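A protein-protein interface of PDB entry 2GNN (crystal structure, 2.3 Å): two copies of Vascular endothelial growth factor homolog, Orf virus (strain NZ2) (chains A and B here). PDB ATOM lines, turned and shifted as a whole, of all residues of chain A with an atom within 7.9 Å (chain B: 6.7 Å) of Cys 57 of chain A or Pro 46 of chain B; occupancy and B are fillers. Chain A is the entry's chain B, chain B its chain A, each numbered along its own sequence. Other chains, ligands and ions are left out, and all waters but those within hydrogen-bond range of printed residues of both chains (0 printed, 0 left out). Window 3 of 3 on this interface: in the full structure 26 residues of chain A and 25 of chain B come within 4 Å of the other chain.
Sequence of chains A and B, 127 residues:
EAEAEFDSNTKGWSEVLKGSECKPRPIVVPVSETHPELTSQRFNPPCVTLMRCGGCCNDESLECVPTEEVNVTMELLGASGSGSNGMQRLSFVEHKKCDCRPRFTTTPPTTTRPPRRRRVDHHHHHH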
ATOM      1  N   VAL A  16      32.583  -9.550  -6.717  1.00  0.00           N
ATOM      2  CA  VAL A  16      31.705 -10.204  -7.697  1.00  0.00           C
ATOM      3  C   VAL A  16      30.319 -10.451  -7.098  1.00  0.00           C
ATOM      4  O   VAL A  16      29.293 -10.168  -7.728  1.00  0.00           O
ATOM      5  CB  VAL A  16      32.313 -11.536  -8.236  1.00  0.00           C
ATOM      6  CG1 VAL A  16      31.342 -12.230  -9.184  1.00  0.00           C
ATOM      7  CG2 VAL A  16      33.625 -11.279  -8.951  1.00  0.00           C
ATOM      8  N   LEU A  17      30.310 -10.972  -5.873  1.00  0.00           N
ATOM      9  CA  LEU A  17      29.089 -11.224  -5.122  1.00  0.00           C
ATOM     10  C   LEU A  17      28.308  -9.933  -4.909  1.00  0.00           C
ATOM     11  O   LEU A  17      27.127  -9.855  -5.242  1.00  0.00           O
ATOM     12  CB  LEU A  17      29.435 -11.878  -3.787  1.00  0.00           C
ATOM     13  CG  LEU A  17      28.275 -12.311  -2.897  1.00  0.00           C
ATOM     14  CD1 LEU A  17      27.658 -13.611  -3.410  1.00  0.00           C
ATOM     15  CD2 LEU A  17      28.760 -12.455  -1.468  1.00  0.00           C
ATOM     16  N   SER A  20      26.396  -8.868  -7.863  1.00  0.00           N
ATOM     17  CA  SER A  20      25.267  -9.712  -8.277  1.00  0.00           C
ATOM     18  C   SER A  20      24.087  -9.754  -7.283  1.00  0.00           C
ATOM     19  O   SER A  20      23.070 -10.413  -7.549  1.00  0.00           O
ATOM     20  CB  SER A  20      25.738 -11.134  -8.529  1.00  0.00           C
ATOM     21  OG  SER A  20      25.863 -11.825  -7.308  1.00  0.00           O
ATOM     22  N   GLU A  21      24.212  -9.053  -6.158  1.00  0.00           N
ATOM     23  CA  GLU A  21      23.185  -9.110  -5.116  1.00  0.00           C
ATOM     24  C   GLU A  21      21.886  -8.421  -5.525  1.00  0.00           C
ATOM     25  O   GLU A  21      21.877  -7.538  -6.390  1.00  0.00           O
ATOM     26  CB  GLU A  21      23.708  -8.626  -3.751  1.00  0.00           C
ATOM     27  CG  GLU A  21      24.182  -7.176  -3.677  1.00  0.00           C
ATOM     28  CD  GLU A  21      24.675  -6.790  -2.279  1.00  0.00           C
ATOM     29  OE1 GLU A  21      25.279  -7.645  -1.582  1.00  0.00           O
ATOM     30  OE2 GLU A  21      24.453  -5.625  -1.875  1.00  0.00           O
ATOM     31  N   CYS A  22      20.791  -8.871  -4.916  1.00  0.00           N
ATOM     32  CA  CYS A  22      19.469  -8.292  -5.108  1.00  0.00           C
ATOM     33  C   CYS A  22      19.434  -6.928  -4.435  1.00  0.00           C
ATOM     34  O   CYS A  22      19.521  -6.826  -3.218  1.00  0.00           O
ATOM     35  CB  CYS A  22      18.408  -9.217  -4.505  1.00  0.00           C
ATOM     36  SG  CYS A  22      16.756  -8.520  -4.426  1.00  0.00           S
ATOM     37  N   GLY A  54      16.959  -5.609  -8.952  1.00  0.00           N
ATOM     38  CA  GLY A  54      17.679  -6.472  -9.883  1.00  0.00           C
ATOM     39  C   GLY A  54      18.804  -7.204  -9.178  1.00  0.00           C
ATOM     40  O   GLY A  54      19.235  -6.805  -8.092  1.00  0.00           O
ATOM     41  N   GLY A  55      19.277  -8.276  -9.797  1.00  0.00           N
ATOM     42  CA  GLY A  55      20.261  -9.126  -9.170  1.00  0.00           C
ATOM     43  C   GLY A  55      19.841 -10.569  -9.250  1.00  0.00           C
ATOM     44  O   GLY A  55      18.908 -10.918  -9.975  1.00  0.00           O
ATOM     45  N   CYS A  56      20.555 -11.401  -8.511  1.00  0.00           N
ATOM     46  CA  CYS A  56      20.323 -12.825  -8.456  1.00  0.00           C
ATOM     47  C   CYS A  56      20.066 -13.251  -7.026  1.00  0.00           C
ATOM     48  O   CYS A  56      20.791 -12.848  -6.104  1.00  0.00           O
ATOM     49  CB  CYS A  56      21.568 -13.567  -8.940  1.00  0.00           C
ATOM     50  SG  CYS A  56      21.584 -13.784 -10.693  1.00  0.00           S
ATOM     51  N   CYS A  57      19.051 -14.086  -6.841  1.00  0.00           N
ATOM     52  CA  CYS A  57      18.861 -14.740  -5.553  1.00  0.00           C
ATOM     53  C   CYS A  57      19.618 -16.062  -5.545  1.00  0.00           C
ATOM     54  O   CYS A  57      19.813 -16.687  -6.588  1.00  0.00           O
ATOM     55  CB  CYS A  57      17.375 -14.926  -5.247  1.00  0.00           C
ATOM     56  SG  CYS A  57      16.481 -13.357  -5.109  1.00  0.00           S
ATOM     57  N   ASN A  58      20.046 -16.476  -4.360  1.00  0.00           N
ATOM     58  CA  ASN A  58      20.843 -17.683  -4.187  1.00  0.00           C
ATOM     59  C   ASN A  58      20.064 -18.987  -4.404  1.00  0.00           C
ATOM     60  O   ASN A  58      20.595 -20.079  -4.169  1.00  0.00           O
ATOM     61  CB  ASN A  58      21.468 -17.675  -2.780  1.00  0.00           C
ATOM     62  CG  ASN A  58      20.487 -17.204  -1.702  1.00  0.00           C
ATOM     63  OD1 ASN A  58      19.761 -16.214  -1.886  1.00  0.00           O
ATOM     64  ND2 ASN A  58      20.465 -17.911  -0.574  1.00  0.00           N
ATOM     65  N   ASP A  59      18.814 -18.877  -4.846  1.00  0.00           N
ATOM     66  CA  ASP A  59      17.903 -20.018  -4.893  1.00  0.00           C
ATOM     67  C   ASP A  59      16.879 -19.829  -5.994  1.00  0.00           C
ATOM     68  O   ASP A  59      16.259 -18.771  -6.098  1.00  0.00           O
ATOM     69  CB  ASP A  59      17.189 -20.163  -3.540  1.00  0.00           C
ATOM     70  CG  ASP A  59      16.517 -21.520  -3.354  1.00  0.00           C
ATOM     71  OD1 ASP A  59      15.558 -21.842  -4.093  1.00  0.00           O
ATOM     72  OD2 ASP A  59      16.937 -22.251  -2.431  1.00  0.00           O
ATOM     73  N   GLU A  60      16.695 -20.876  -6.795  1.00  0.00           N
ATOM     74  CA  GLU A  60      15.735 -20.895  -7.905  1.00  0.00           C
ATOM     75  C   GLU A  60      14.296 -20.552  -7.481  1.00  0.00           C
ATOM     76  O   GLU A  60      13.501 -20.082  -8.294  1.00  0.00           O
ATOM     77  CB  GLU A  60      15.772 -22.279  -8.571  1.00  0.00           C
ATOM     78  CG  GLU A  60      14.855 -22.452  -9.791  1.00  0.00           C
ATOM     79  CD  GLU A  60      14.213 -23.839  -9.855  1.00  0.00           C
ATOM     80  OE1 GLU A  60      14.741 -24.793  -9.228  1.00  0.00           O
ATOM     81  OE2 GLU A  60      13.171 -23.968 -10.539  1.00  0.00           O
ATOM     82  N   SER A  61      13.971 -20.796  -6.210  1.00  0.00           N
ATOM     83  CA  SER A  61      12.620 -20.574  -5.678  1.00  0.00           C
ATOM     84  C   SER A  61      12.412 -19.155  -5.137  1.00  0.00           C
ATOM     85  O   SER A  61      11.346 -18.842  -4.596  1.00  0.00           O
ATOM     86  CB  SER A  61      12.307 -21.598  -4.586  1.00  0.00           C
ATOM     87  OG  SER A  61      12.830 -22.872  -4.916  1.00  0.00           O
ATOM     88  N   LEU A  62      13.426 -18.303  -5.290  1.00  0.00           N
ATOM     89  CA  LEU A  62      13.375 -16.930  -4.791  1.00  0.00           C
ATOM     90  C   LEU A  62      13.427 -15.899  -5.928  1.00  0.00           C
ATOM     91  O   LEU A  62      14.050 -16.124  -6.961  1.00  0.00           O
ATOM     92  CB  LEU A  62      14.494 -16.677  -3.764  1.00  0.00           C
ATOM     93  CG  LEU A  62      14.458 -17.459  -2.441  1.00  0.00           C
ATOM     94  CD1 LEU A  62      15.741 -17.315  -1.638  1.00  0.00           C
ATOM     95  CD2 LEU A  62      13.295 -17.007  -1.603  1.00  0.00           C
ATOM     96  N   GLU A  63      12.748 -14.777  -5.731  1.00  0.00           N
ATOM     97  CA  GLU A  63      12.788 -13.687  -6.676  1.00  0.00           C
ATOM     98  C   GLU A  63      13.122 -12.382  -5.978  1.00  0.00           C
ATOM     99  O   GLU A  63      12.793 -12.180  -4.809  1.00  0.00           O
ATOM    100  CB  GLU A  63      11.475 -13.570  -7.458  1.00  0.00           C
ATOM    101  CG  GLU A  63      10.203 -13.615  -6.604  1.00  0.00           C
ATOM    102  CD  GLU A  63       8.931 -13.452  -7.427  1.00  0.00           C
ATOM    103  OE1 GLU A  63       9.035 -13.185  -8.643  1.00  0.00           O
ATOM    104  OE2 GLU A  63       7.824 -13.592  -6.854  1.00  0.00           O
ATOM    105  N   CYS A  64      13.793 -11.509  -6.717  1.00  0.00           N
ATOM    106  CA  CYS A  64      14.262 -10.246  -6.195  1.00  0.00           C
ATOM    107  C   CYS A  64      13.170  -9.227  -6.442  1.00  0.00           C
ATOM    108  O   CYS A  64      12.883  -8.893  -7.586  1.00  0.00           O
ATOM    109  CB  CYS A  64      15.572  -9.853  -6.891  1.00  0.00           C
ATOM    110  SG  CYS A  64      16.248  -8.276  -6.363  1.00  0.00           S
ATOM    111  N   VAL A  65      12.550  -8.757  -5.367  1.00  0.00           N
ATOM    112  CA  VAL A  65      11.358  -7.913  -5.480  1.00  0.00           C
ATOM    113  C   VAL A  65      11.464  -6.704  -4.555  1.00  0.00           C
ATOM    114  O   VAL A  65      12.191  -6.754  -3.560  1.00  0.00           O
ATOM    115  CB  VAL A  65      10.062  -8.707  -5.147  1.00  0.00           C
ATOM    116  CG1 VAL A  65       9.816  -9.806  -6.165  1.00  0.00           C
ATOM    117  CG2 VAL A  65      10.130  -9.295  -3.756  1.00  0.00           C
ATOM    118  N   ASP A  99      14.334  -7.438  -1.800  1.00  0.00           N
ATOM    119  CA  ASP A  99      14.577  -8.630  -0.992  1.00  0.00           C
ATOM    120  C   ASP A  99      14.362  -9.895  -1.814  1.00  0.00           C
ATOM    121  O   ASP A  99      13.611  -9.899  -2.790  1.00  0.00           O
ATOM    122  CB  ASP A  99      13.666  -8.605   0.248  1.00  0.00           C
ATOM    123  CG  ASP A  99      14.233  -9.381   1.429  1.00  0.00           C
ATOM    124  OD1 ASP A  99      15.432  -9.738   1.428  1.00  0.00           O
ATOM    125  OD2 ASP A  99      13.458  -9.627   2.382  1.00  0.00           O
ATOM    126  N   CYS A 100      15.051 -10.960  -1.425  1.00  0.00           N
ATOM    127  CA  CYS A 100      14.836 -12.272  -2.025  1.00  0.00           C
ATOM    128  C   CYS A 100      13.721 -13.018  -1.272  1.00  0.00           C
ATOM    129  O   CYS A 100      13.916 -13.522  -0.156  1.00  0.00           O
ATOM    130  CB  CYS A 100      16.148 -13.073  -2.093  1.00  0.00           C
ATOM    131  SG  CYS A 100      17.267 -12.521  -3.433  1.00  0.00           S
ATOM    132  N   ARG A 101      12.556 -13.059  -1.916  1.00  0.00           N
ATOM    133  CA  ARG A 101      11.308 -13.555  -1.347  1.00  0.00           C
ATOM    134  C   ARG A 101      10.799 -14.739  -2.178  1.00  0.00           C
ATOM    135  O   ARG A 101      11.014 -14.771  -3.392  1.00  0.00           O
ATOM    136  CB  ARG A 101      10.258 -12.432  -1.354  1.00  0.00           C
ATOM    137  CG  ARG A 101      10.635 -11.175  -0.561  1.00  0.00           C
ATOM    138  CD  ARG A 101      10.571 -11.409   0.945  1.00  0.00           C
ATOM    139  NE  ARG A 101      10.819 -10.198   1.732  1.00  0.00           N
ATOM    140  CZ  ARG A 101       9.889  -9.301   2.074  1.00  0.00           C
ATOM    141  NH1 ARG A 101       8.624  -9.452   1.690  1.00  0.00           N
ATOM    142  NH2 ARG A 101      10.229  -8.242   2.801  1.00  0.00           N
ATOM    143  N   PRO A 102      10.124 -15.713  -1.536  1.00  0.00           N
ATOM    144  CA  PRO A 102       9.615 -16.888  -2.255  1.00  0.00           C
ATOM    145  C   PRO A 102       8.559 -16.514  -3.295  1.00  0.00           C
ATOM    146  O   PRO A 102       7.932 -15.462  -3.175  1.00  0.00           O
ATOM    147  CB  PRO A 102       8.978 -17.732  -1.143  1.00  0.00           C
ATOM    148  CG  PRO A 102       9.558 -17.212   0.123  1.00  0.00           C
ATOM    149  CD  PRO A 102       9.787 -15.769  -0.102  1.00  0.00           C
ATOM    150  N   ARG A 103       8.364 -17.366  -4.301  1.00  0.00           N
ATOM    151  CA  ARG A 103       7.354 -17.118  -5.342  1.00  0.00           C
ATOM    152  C   ARG A 103       5.942 -17.551  -4.938  1.00  0.00           C
ATOM    153  O   ARG A 103       4.957 -17.180  -5.591  1.00  0.00           O
ATOM    154  CB  ARG A 103       7.739 -17.801  -6.652  1.00  0.00           C
ATOM    155  CG  ARG A 103       8.846 -17.105  -7.393  1.00  0.00           C
ATOM    156  CD  ARG A 103       8.856 -17.488  -8.865  1.00  0.00           C
ATOM    157  NE  ARG A 103       9.992 -16.874  -9.550  1.00  0.00           N
ATOM    158  CZ  ARG A 103      11.242 -17.332  -9.495  1.00  0.00           C
ATOM    159  NH1 ARG A 103      11.531 -18.422  -8.787  1.00  0.00           N
ATOM    160  NH2 ARG A 103      12.207 -16.698 -10.149  1.00  0.00           N
ATOM    161  N   VAL B  29      23.792 -10.293 -15.740  1.00  0.00           N
ATOM    162  CA  VAL B  29      23.853 -11.343 -16.736  1.00  0.00           C
ATOM    163  C   VAL B  29      24.034 -12.680 -16.051  1.00  0.00           C
ATOM    164  O   VAL B  29      24.945 -12.840 -15.238  1.00  0.00           O
ATOM    165  CB  VAL B  29      25.022 -11.113 -17.730  1.00  0.00           C
ATOM    166  CG1 VAL B  29      24.931 -12.089 -18.869  1.00  0.00           C
ATOM    167  CG2 VAL B  29      25.001  -9.704 -18.285  1.00  0.00           C
ATOM    168  N   PRO B  30      23.157 -13.650 -16.359  1.00  0.00           N
ATOM    169  CA  PRO B  30      23.309 -15.001 -15.829  1.00  0.00           C
ATOM    170  C   PRO B  30      24.550 -15.675 -16.391  1.00  0.00           C
ATOM    171  O   PRO B  30      24.792 -15.604 -17.592  1.00  0.00           O
ATOM    172  CB  PRO B  30      22.045 -15.720 -16.317  1.00  0.00           C
ATOM    173  CG  PRO B  30      21.099 -14.630 -16.713  1.00  0.00           C
ATOM    174  CD  PRO B  30      21.963 -13.526 -17.209  1.00  0.00           C
ATOM    175  N   VAL B  31      25.327 -16.317 -15.526  1.00  0.00           N
ATOM    176  CA  VAL B  31      26.562 -16.984 -15.938  1.00  0.00           C
ATOM    177  C   VAL B  31      26.302 -18.087 -16.972  1.00  0.00           C
ATOM    178  O   VAL B  31      27.065 -18.234 -17.929  1.00  0.00           O
ATOM    179  CB  VAL B  31      27.349 -17.551 -14.726  1.00  0.00           C
ATOM    180  CG1 VAL B  31      28.638 -18.198 -15.184  1.00  0.00           C
ATOM    181  CG2 VAL B  31      27.656 -16.453 -13.727  1.00  0.00           C
ATOM    182  N   SER B  32      25.216 -18.837 -16.784  1.00  0.00           N
ATOM    183  CA  SER B  32      24.865 -19.955 -17.670  1.00  0.00           C
ATOM    184  C   SER B  32      24.547 -19.533 -19.118  1.00  0.00           C
ATOM    185  O   SER B  32      24.672 -20.342 -20.039  1.00  0.00           O
ATOM    186  CB  SER B  32      23.722 -20.793 -17.071  1.00  0.00           C
ATOM    187  OG  SER B  32      22.539 -20.027 -16.916  1.00  0.00           O
ATOM    188  N   ARG B  42      26.617 -25.173 -11.677  1.00  0.00           N
ATOM    189  CA  ARG B  42      26.024 -23.988 -11.052  1.00  0.00           C
ATOM    190  C   ARG B  42      27.135 -23.155 -10.416  1.00  0.00           C
ATOM    191  O   ARG B  42      28.130 -23.704  -9.927  1.00  0.00           O
ATOM    192  CB  ARG B  42      25.000 -24.375  -9.981  1.00  0.00           C
ATOM    193  CG  ARG B  42      24.105 -25.554 -10.330  1.00  0.00           C
ATOM    194  CD  ARG B  42      23.317 -26.005  -9.113  1.00  0.00           C
ATOM    195  NE  ARG B  42      23.070 -27.446  -9.115  1.00  0.00           N
ATOM    196  CZ  ARG B  42      23.893 -28.358  -8.596  1.00  0.00           C
ATOM    197  NH1 ARG B  42      25.037 -27.992  -8.030  1.00  0.00           N
ATOM    198  NH2 ARG B  42      23.572 -29.643  -8.645  1.00  0.00           N
ATOM    199  N   PHE B  43      26.957 -21.834 -10.424  1.00  0.00           N
ATOM    200  CA  PHE B  43      27.956 -20.908  -9.887  1.00  0.00           C
ATOM    201  C   PHE B  43      27.421 -20.011  -8.783  1.00  0.00           C
ATOM    202  O   PHE B  43      26.289 -19.534  -8.850  1.00  0.00           O
ATOM    203  CB  PHE B  43      28.546 -20.037 -11.000  1.00  0.00           C
ATOM    204  CG  PHE B  43      29.537 -20.753 -11.855  1.00  0.00           C
ATOM    205  CD1 PHE B  43      30.799 -21.075 -11.359  1.00  0.00           C
ATOM    206  CD2 PHE B  43      29.212 -21.121 -13.155  1.00  0.00           C
ATOM    207  CE1 PHE B  43      31.725 -21.752 -12.146  1.00  0.00           C
ATOM    208  CE2 PHE B  43      30.130 -21.793 -13.954  1.00  0.00           C
ATOM    209  CZ  PHE B  43      31.390 -22.112 -13.447  1.00  0.00           C
ATOM    210  N   ASN B  44      28.257 -19.788  -7.775  1.00  0.00           N
ATOM    211  CA  ASN B  44      27.966 -18.838  -6.717  1.00  0.00           C
ATOM    212  C   ASN B  44      28.898 -17.632  -6.848  1.00  0.00           C
ATOM    213  O   ASN B  44      30.101 -17.753  -6.600  1.00  0.00           O
ATOM    214  CB  ASN B  44      28.127 -19.508  -5.345  1.00  0.00           C
ATOM    215  CG  ASN B  44      27.507 -18.704  -4.212  1.00  0.00           C
ATOM    216  OD1 ASN B  44      27.351 -17.487  -4.301  1.00  0.00           O
ATOM    217  ND2 ASN B  44      27.156 -19.391  -3.132  1.00  0.00           N
ATOM    218  N   PRO B  45      28.358 -16.465  -7.250  1.00  0.00           N
ATOM    219  CA  PRO B  45      26.974 -16.156  -7.631  1.00  0.00           C
ATOM    220  C   PRO B  45      26.573 -16.622  -9.046  1.00  0.00           C
ATOM    221  O   PRO B  45      27.434 -16.758  -9.912  1.00  0.00           O
ATOM    222  CB  PRO B  45      26.935 -14.630  -7.548  1.00  0.00           C
ATOM    223  CG  PRO B  45      28.325 -14.205  -7.872  1.00  0.00           C
ATOM    224  CD  PRO B  45      29.220 -15.269  -7.305  1.00  0.00           C
ATOM    225  N   PRO B  46      25.267 -16.890  -9.267  1.00  0.00           N
ATOM    226  CA  PRO B  46      24.755 -17.378 -10.558  1.00  0.00           C
ATOM    227  C   PRO B  46      24.685 -16.330 -11.654  1.00  0.00           C
ATOM    228  O   PRO B  46      24.265 -16.631 -12.778  1.00  0.00           O
ATOM    229  CB  PRO B  46      23.348 -17.861 -10.210  1.00  0.00           C
ATOM    230  CG  PRO B  46      22.952 -17.055  -9.031  1.00  0.00           C
ATOM    231  CD  PRO B  46      24.201 -16.805  -8.249  1.00  0.00           C
ATOM    232  N   CYS B  47      25.073 -15.103 -11.324  1.00  0.00           N
ATOM    233  CA  CYS B  47      25.148 -14.048 -12.300  1.00  0.00           C
ATOM    234  C   CYS B  47      26.113 -12.934 -11.903  1.00  0.00           C
ATOM    235  O   CYS B  47      26.573 -12.881 -10.769  1.00  0.00           O
ATOM    236  CB  CYS B  47      23.763 -13.499 -12.599  1.00  0.00           C
ATOM    237  SG  CYS B  47      23.072 -12.560 -11.316  1.00  0.00           S
ATOM    238  N   VAL B  48      26.417 -12.055 -12.857  1.00  0.00           N
ATOM    239  CA  VAL B  48      27.395 -10.989 -12.663  1.00  0.00           C
ATOM    240  C   VAL B  48      26.894  -9.694 -13.266  1.00  0.00           C
ATOM    241  O   VAL B  48      26.047  -9.713 -14.158  1.00  0.00           O
ATOM    242  CB  VAL B  48      28.772 -11.343 -13.305  1.00  0.00           C
ATOM    243  CG1 VAL B  48      29.374 -12.562 -12.639  1.00  0.00           C
ATOM    244  CG2 VAL B  48      28.646 -11.566 -14.812  1.00  0.00           C
ATOM    245  N   LEU B  76      34.665 -16.811  -9.270  1.00  0.00           N
ATOM    246  CA  LEU B  76      33.338 -17.339  -8.942  1.00  0.00           C
ATOM    247  C   LEU B  76      33.460 -18.715  -8.311  1.00  0.00           C
ATOM    248  O   LEU B  76      34.341 -19.483  -8.675  1.00  0.00           O
ATOM    249  CB  LEU B  76      32.464 -17.447 -10.191  1.00  0.00           C
ATOM    250  CG  LEU B  76      31.821 -16.179 -10.752  1.00  0.00           C
ATOM    251  CD1 LEU B  76      32.697 -15.551 -11.808  1.00  0.00           C
ATOM    252  CD2 LEU B  76      30.475 -16.510 -11.346  1.00  0.00           C
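No position is printed for both chains.
Of the 8 pairs that touch across the chains among the printed residues, none has its exchanged pair printed and touching as well.
The backbone NH of Val 29 of chain B lies within hydrogen-bond range of the backbone carbonyl oxygen of Val 48 of chain B (2.8 Å).
The side-chain sulfur (SG) of Cys 100 of chain A is disulfide-bonded to the side-chain sulfur (SG) of Cys 57 of chain A.
N of Val 31 of chain B sits at hydrogen-bond distance from O of Pro 46 of chain B, at 3.0 Å.
SG of Cys 64 of chain A forms a disulfide with SG of Cys 22 of chain A (2.0 Å).
The backbone carbonyl oxygen (O) of Leu 17 of chain A lies within hydrogen-bond range of the side-chain hydroxyl (OG) of Ser 20 of chain A, at 3.1 Å.
The backbone NH of Cys 56 of chain A lies within hydrogen-bond range of the backbone carbonyl oxygen of Ser 20 of chain A.
Of the printed residues of chain B, Cys 57 of chain A touches Pro 46 (3.99 Å).
Of the printed residues of chain A, Pro 46 of chain B touches Cys 56 and Cys 57.
Printed residues of chain B within 4 Å of Cys 56 of chain A: Pro 46 (3.8 Å) and Cys 47 (2.0 Å).
Printed residues of chain B within 4 Å of Val 16 of chain A: Pro 45 and Val 48.
Of the printed residues of chain B, Leu 17 of chain A touches Asn 44.
Of the printed residues of chain A, Asn 44 of chain B touches Leu 17.
Of the printed residues of chain A, Val 48 of chain B touches Val 16.
The nearest printed residue of chain B that does not touch Cys 57 of chain A is Cys 47 of chain B (6.2 Å).
The nearest printed residue of chain A that does not touch Pro 46 of chain B is Asn 58 of chain A (5.3 Å).
Pro 45 of chain B touches Val 16 of chain A (CG to CG1, 3.8 Å).
CG1 of Val 48 of chain B touches CG1 of Val 16 of chain A (3.99 Å).
Leu 17 of chain A touches Asn 44 of chain B (CD1 to OD1, 3.99 Å).
Ser 20 of chain A touches Pro 45 of chain B (OG to CB, 3.0 Å).
CB of Ser 20 of chain A touches O of Cys 47 of chain B, 3.0 Å away.
Cys 56 of chain A touches Pro 46 of chain B.
Pro 46 of chain B touches Cys 57 of chain A.
Hydrophobic or aromatic side chains of chain B within 4 Å of the printed part of chain A: Pro 45, Pro 46 and Val 48.
SG of Cys 56 of chain A is disulfide-bonded to SG of Cys 47 of chain B, 2.0 Å away.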
